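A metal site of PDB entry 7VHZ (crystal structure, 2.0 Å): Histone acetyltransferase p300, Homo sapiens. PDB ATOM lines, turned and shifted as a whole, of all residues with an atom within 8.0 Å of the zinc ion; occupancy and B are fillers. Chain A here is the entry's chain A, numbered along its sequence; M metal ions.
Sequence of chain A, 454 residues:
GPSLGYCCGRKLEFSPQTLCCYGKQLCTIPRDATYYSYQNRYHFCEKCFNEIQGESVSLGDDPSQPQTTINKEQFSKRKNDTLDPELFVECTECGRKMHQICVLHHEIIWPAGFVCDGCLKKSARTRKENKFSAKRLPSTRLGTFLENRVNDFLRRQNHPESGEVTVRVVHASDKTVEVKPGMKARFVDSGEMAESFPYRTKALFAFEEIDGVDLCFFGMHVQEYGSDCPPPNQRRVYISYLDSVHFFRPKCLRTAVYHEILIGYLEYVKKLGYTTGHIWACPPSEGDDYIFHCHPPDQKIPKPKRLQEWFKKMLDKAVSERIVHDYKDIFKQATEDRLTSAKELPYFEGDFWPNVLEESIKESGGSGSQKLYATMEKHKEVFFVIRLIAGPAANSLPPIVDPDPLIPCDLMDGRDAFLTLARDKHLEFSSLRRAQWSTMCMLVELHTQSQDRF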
ATOM      1  N   TYR A   6      20.889 -14.655  30.636  1.00  0.00           N
ATOM      2  CA  TYR A   6      20.030 -15.684  30.058  1.00  0.00           C
ATOM      3  C   TYR A   6      20.649 -17.074  30.172  1.00  0.00           C
ATOM      4  O   TYR A   6      21.770 -17.227  30.666  1.00  0.00           O
ATOM      5  CB  TYR A   6      19.719 -15.368  28.595  1.00  0.00           C
ATOM      6  N   CYS A   7      19.878 -18.081  29.774  1.00  0.00           N
ATOM      7  CA  CYS A   7      20.242 -19.490  29.957  1.00  0.00           C
ATOM      8  C   CYS A   7      21.307 -19.971  28.973  1.00  0.00           C
ATOM      9  O   CYS A   7      22.424 -20.316  29.371  1.00  0.00           O
ATOM     10  CB  CYS A   7      18.988 -20.362  29.827  1.00  0.00           C
ATOM     11  SG  CYS A   7      18.186 -20.409  28.203  1.00  0.00           S
ATOM     12  N   CYS A   8      20.976 -19.973  27.676  1.00  0.00           N
ATOM     13  CA  CYS A   8      21.869 -20.425  26.618  1.00  0.00           C
ATOM     14  C   CYS A   8      22.719 -19.307  26.040  1.00  0.00           C
ATOM     15  O   CYS A   8      23.408 -19.515  25.045  1.00  0.00           O
ATOM     16  CB  CYS A   8      21.041 -21.063  25.495  1.00  0.00           C
ATOM     17  SG  CYS A   8      19.826 -19.901  24.738  1.00  0.00           S
ATOM     18  N   GLY A   9      22.680 -18.129  26.657  1.00  0.00           N
ATOM     19  CA  GLY A   9      23.490 -16.999  26.223  1.00  0.00           C
ATOM     20  C   GLY A   9      23.023 -16.338  24.947  1.00  0.00           C
ATOM     21  O   GLY A   9      23.780 -15.587  24.345  1.00  0.00           O
ATOM     22  N   ARG A  10      21.788 -16.585  24.534  1.00  0.00           N
ATOM     23  CA  ARG A  10      21.278 -16.108  23.262  1.00  0.00           C
ATOM     24  C   ARG A  10      20.111 -15.162  23.504  1.00  0.00           C
ATOM     25  O   ARG A  10      19.211 -15.469  24.300  1.00  0.00           O
ATOM     26  CB  ARG A  10      20.874 -17.261  22.346  1.00  0.00           C
ATOM     27  CG  ARG A  10      21.871 -17.516  21.224  1.00  0.00           C
ATOM     28  CD  ARG A  10      21.578 -18.790  20.475  1.00  0.00           C
ATOM     29  NE  ARG A  10      20.931 -18.530  19.195  1.00  0.00           N
ATOM     30  CZ  ARG A  10      19.954 -19.280  18.683  1.00  0.00           C
ATOM     31  NH1 ARG A  10      19.498 -20.346  19.312  1.00  0.00           N
ATOM     32  NH2 ARG A  10      19.430 -18.941  17.508  1.00  0.00           N
ATOM     33  N   LYS A  11      20.131 -14.016  22.832  1.00  0.00           N
ATOM     34  CA  LYS A  11      19.009 -13.085  22.854  1.00  0.00           C
ATOM     35  C   LYS A  11      18.042 -13.493  21.745  1.00  0.00           C
ATOM     36  O   LYS A  11      18.363 -13.367  20.560  1.00  0.00           O
ATOM     37  CB  LYS A  11      19.493 -11.649  22.658  1.00  0.00           C
ATOM     38  N   LEU A  12      16.865 -13.956  22.139  1.00  0.00           N
ATOM     39  CA  LEU A  12      15.924 -14.599  21.229  1.00  0.00           C
ATOM     40  C   LEU A  12      14.626 -13.811  21.174  1.00  0.00           C
ATOM     41  O   LEU A  12      14.081 -13.435  22.222  1.00  0.00           O
ATOM     42  CB  LEU A  12      15.651 -16.043  21.657  1.00  0.00           C
ATOM     43  CG  LEU A  12      16.896 -16.930  21.663  1.00  0.00           C
ATOM     44  CD1 LEU A  12      16.609 -18.293  22.294  1.00  0.00           C
ATOM     45  CD2 LEU A  12      17.419 -17.092  20.247  1.00  0.00           C
ATOM     46  N   GLU A  86      11.246 -13.587  23.258  1.00  0.00           N
ATOM     47  CA  GLU A  86      10.936 -14.901  23.811  1.00  0.00           C
ATOM     48  C   GLU A  86      10.732 -14.805  25.319  1.00  0.00           C
ATOM     49  O   GLU A  86      11.321 -13.965  26.006  1.00  0.00           O
ATOM     50  CB  GLU A  86      12.027 -15.914  23.480  1.00  0.00           C
ATOM     51  CG  GLU A  86      11.840 -16.613  22.137  1.00  0.00           C
ATOM     52  CD  GLU A  86      12.573 -17.946  22.047  1.00  0.00           C
ATOM     53  OE1 GLU A  86      12.898 -18.527  23.108  1.00  0.00           O
ATOM     54  OE2 GLU A  86      12.832 -18.413  20.932  1.00  0.00           O
ATOM     55  N   LEU A  87       9.878 -15.683  25.840  1.00  0.00           N
ATOM     56  CA  LEU A  87       9.533 -15.682  27.246  1.00  0.00           C
ATOM     57  C   LEU A  87      10.504 -16.536  28.049  1.00  0.00           C
ATOM     58  O   LEU A  87      11.017 -17.551  27.568  1.00  0.00           O
ATOM     59  CB  LEU A  87       8.112 -16.195  27.460  1.00  0.00           C
ATOM     60  CG  LEU A  87       6.960 -15.508  26.723  1.00  0.00           C
ATOM     61  CD1 LEU A  87       5.625 -15.938  27.323  1.00  0.00           C
ATOM     62  CD2 LEU A  87       7.113 -13.996  26.793  1.00  0.00           C
ATOM     63  N   PHE A  88      10.732 -16.118  29.293  1.00  0.00           N
ATOM     64  CA  PHE A  88      11.544 -16.857  30.258  1.00  0.00           C
ATOM     65  C   PHE A  88      10.638 -17.472  31.310  1.00  0.00           C
ATOM     66  O   PHE A  88       9.572 -16.939  31.628  1.00  0.00           O
ATOM     67  CB  PHE A  88      12.579 -15.954  30.936  1.00  0.00           C
ATOM     68  CG  PHE A  88      13.672 -15.479  30.022  1.00  0.00           C
ATOM     69  CD1 PHE A  88      13.497 -14.351  29.248  1.00  0.00           C
ATOM     70  CD2 PHE A  88      14.879 -16.157  29.948  1.00  0.00           C
ATOM     71  CE1 PHE A  88      14.508 -13.899  28.411  1.00  0.00           C
ATOM     72  CE2 PHE A  88      15.891 -15.718  29.117  1.00  0.00           C
ATOM     73  CZ  PHE A  88      15.705 -14.582  28.346  1.00  0.00           C
ATOM     74  N   LYS A  97      16.620 -18.047  35.547  1.00  0.00           N
ATOM     75  CA  LYS A  97      15.735 -17.692  34.444  1.00  0.00           C
ATOM     76  C   LYS A  97      16.223 -18.398  33.182  1.00  0.00           C
ATOM     77  O   LYS A  97      17.387 -18.242  32.788  1.00  0.00           O
ATOM     78  CB  LYS A  97      15.689 -16.178  34.248  1.00  0.00           C
ATOM     79  N   MET A  98      15.336 -19.160  32.548  1.00  0.00           N
ATOM     80  CA  MET A  98      15.652 -19.880  31.324  1.00  0.00           C
ATOM     81  C   MET A  98      14.534 -19.691  30.318  1.00  0.00           C
ATOM     82  O   MET A  98      13.359 -19.579  30.688  1.00  0.00           O
ATOM     83  CB  MET A  98      15.865 -21.389  31.586  1.00  0.00           C
ATOM     84  CG  MET A  98      16.716 -21.705  32.823  1.00  0.00           C
ATOM     85  SD  MET A  98      18.338 -22.392  32.432  1.00  0.00           S
ATOM     86  CE  MET A  98      17.917 -24.088  32.067  1.00  0.00           C
ATOM     87  N   HIS A  99      14.895 -19.650  29.035  1.00  0.00           N
ATOM     88  CA  HIS A  99      13.897 -19.626  27.976  1.00  0.00           C
ATOM     89  C   HIS A  99      12.926 -20.782  28.122  1.00  0.00           C
ATOM     90  O   HIS A  99      13.335 -21.947  28.259  1.00  0.00           O
ATOM     91  CB  HIS A  99      14.578 -19.710  26.601  1.00  0.00           C
ATOM     92  CG  HIS A  99      15.391 -18.503  26.250  1.00  0.00           C
ATOM     93  ND1 HIS A  99      16.751 -18.563  26.029  1.00  0.00           N
ATOM     94  CD2 HIS A  99      15.037 -17.213  26.043  1.00  0.00           C
ATOM     95  CE1 HIS A  99      17.196 -17.356  25.733  1.00  0.00           C
ATOM     96  NE2 HIS A  99      16.183 -16.525  25.726  1.00  0.00           N
ATOM     97  N   GLN A 100      11.630 -20.464  28.100  1.00  0.00           N
ATOM     98  CA  GLN A 100      10.600 -21.493  28.199  1.00  0.00           C
ATOM     99  C   GLN A 100      10.756 -22.525  27.091  1.00  0.00           C
ATOM    100  O   GLN A 100      10.526 -23.719  27.315  1.00  0.00           O
ATOM    101  CB  GLN A 100       9.220 -20.831  28.149  1.00  0.00           C
ATOM    102  CG  GLN A 100       8.045 -21.789  28.308  1.00  0.00           C
ATOM    103  CD  GLN A 100       6.715 -21.060  28.445  1.00  0.00           C
ATOM    104  OE1 GLN A 100       6.581 -19.921  27.997  1.00  0.00           O
ATOM    105  NE2 GLN A 100       5.747 -21.705  29.068  1.00  0.00           N
ATOM    106  N   ILE A 101      11.139 -22.081  25.899  1.00  0.00           N
ATOM    107  CA  ILE A 101      11.287 -22.985  24.766  1.00  0.00           C
ATOM    108  C   ILE A 101      12.504 -23.887  24.938  1.00  0.00           C
ATOM    109  O   ILE A 101      12.469 -25.073  24.586  1.00  0.00           O
ATOM    110  CB  ILE A 101      11.355 -22.169  23.451  1.00  0.00           C
ATOM    111  CG1 ILE A 101       9.986 -21.552  23.159  1.00  0.00           C
ATOM    112  CG2 ILE A 101      11.814 -23.048  22.284  1.00  0.00           C
ATOM    113  CD1 ILE A 101       9.966 -20.659  21.940  1.00  0.00           C
ATOM    114  N   CYS A 102      13.593 -23.346  25.507  1.00  0.00           N
ATOM    115  CA  CYS A 102      14.804 -24.144  25.687  1.00  0.00           C
ATOM    116  C   CYS A 102      14.568 -25.307  26.642  1.00  0.00           C
ATOM    117  O   CYS A 102      15.106 -26.395  26.444  1.00  0.00           O
ATOM    118  CB  CYS A 102      15.942 -23.263  26.217  1.00  0.00           C
ATOM    119  SG  CYS A 102      16.694 -22.131  25.022  1.00  0.00           S
ATOM    120  N   VAL A 103      13.763 -25.085  27.686  1.00  0.00           N
ATOM    121  CA  VAL A 103      13.523 -26.113  28.683  1.00  0.00           C
ATOM    122  C   VAL A 103      12.213 -26.845  28.447  1.00  0.00           C
ATOM    123  O   VAL A 103      11.918 -27.809  29.169  1.00  0.00           O
ATOM    124  CB  VAL A 103      13.542 -25.532  30.109  1.00  0.00           C
ATOM    125  CG1 VAL A 103      14.868 -24.836  30.362  1.00  0.00           C
ATOM    126  CG2 VAL A 103      12.370 -24.536  30.306  1.00  0.00           C
ATOM    127  N   ARG A 433      14.363 -26.362  18.106  1.00  0.00           N
ATOM    128  CA  ARG A 433      13.872 -26.058  19.449  1.00  0.00           C
ATOM    129  C   ARG A 433      12.465 -25.484  19.419  1.00  0.00           C
ATOM    130  O   ARG A 433      11.619 -25.874  20.225  1.00  0.00           O
ATOM    131  CB  ARG A 433      14.837 -25.104  20.158  1.00  0.00           C
ATOM    132  CG  ARG A 433      15.096 -23.790  19.443  1.00  0.00           C
ATOM    133  CD  ARG A 433      16.115 -22.941  20.196  1.00  0.00           C
ATOM    134  NE  ARG A 433      15.613 -22.476  21.483  1.00  0.00           N
ATOM    135  CZ  ARG A 433      14.910 -21.369  21.668  1.00  0.00           C
ATOM    136  NH1 ARG A 433      14.600 -20.576  20.657  1.00  0.00           N
ATOM    137  NH2 ARG A 433      14.515 -21.044  22.889  1.00  0.00           N
HETATM  138 ZN    ZN M   1      17.872 -20.349  25.912  1.00  0.00          ZN
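The guanidinium group of Arg 433 lies close to the side-chain sulfur of Cys 102 (3.2 Å).
The zinc ion is bound by a ring nitrogen (ND1) of His 99 (2.1 Å), the side-chain sulfur of Cys 102 (2.3 Å), the side-chain sulfur of Cys 7 (2.3 Å) and the side-chain sulfur of Cys 8 (2.3 Å). The zinc ion has four donor atoms within binding distance.
Of the 18 residues printed, 4 come within 4 Å of the zinc ion. The nearest printed residue that does not touch the zinc ion is Leu 12 (4.3 Å).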
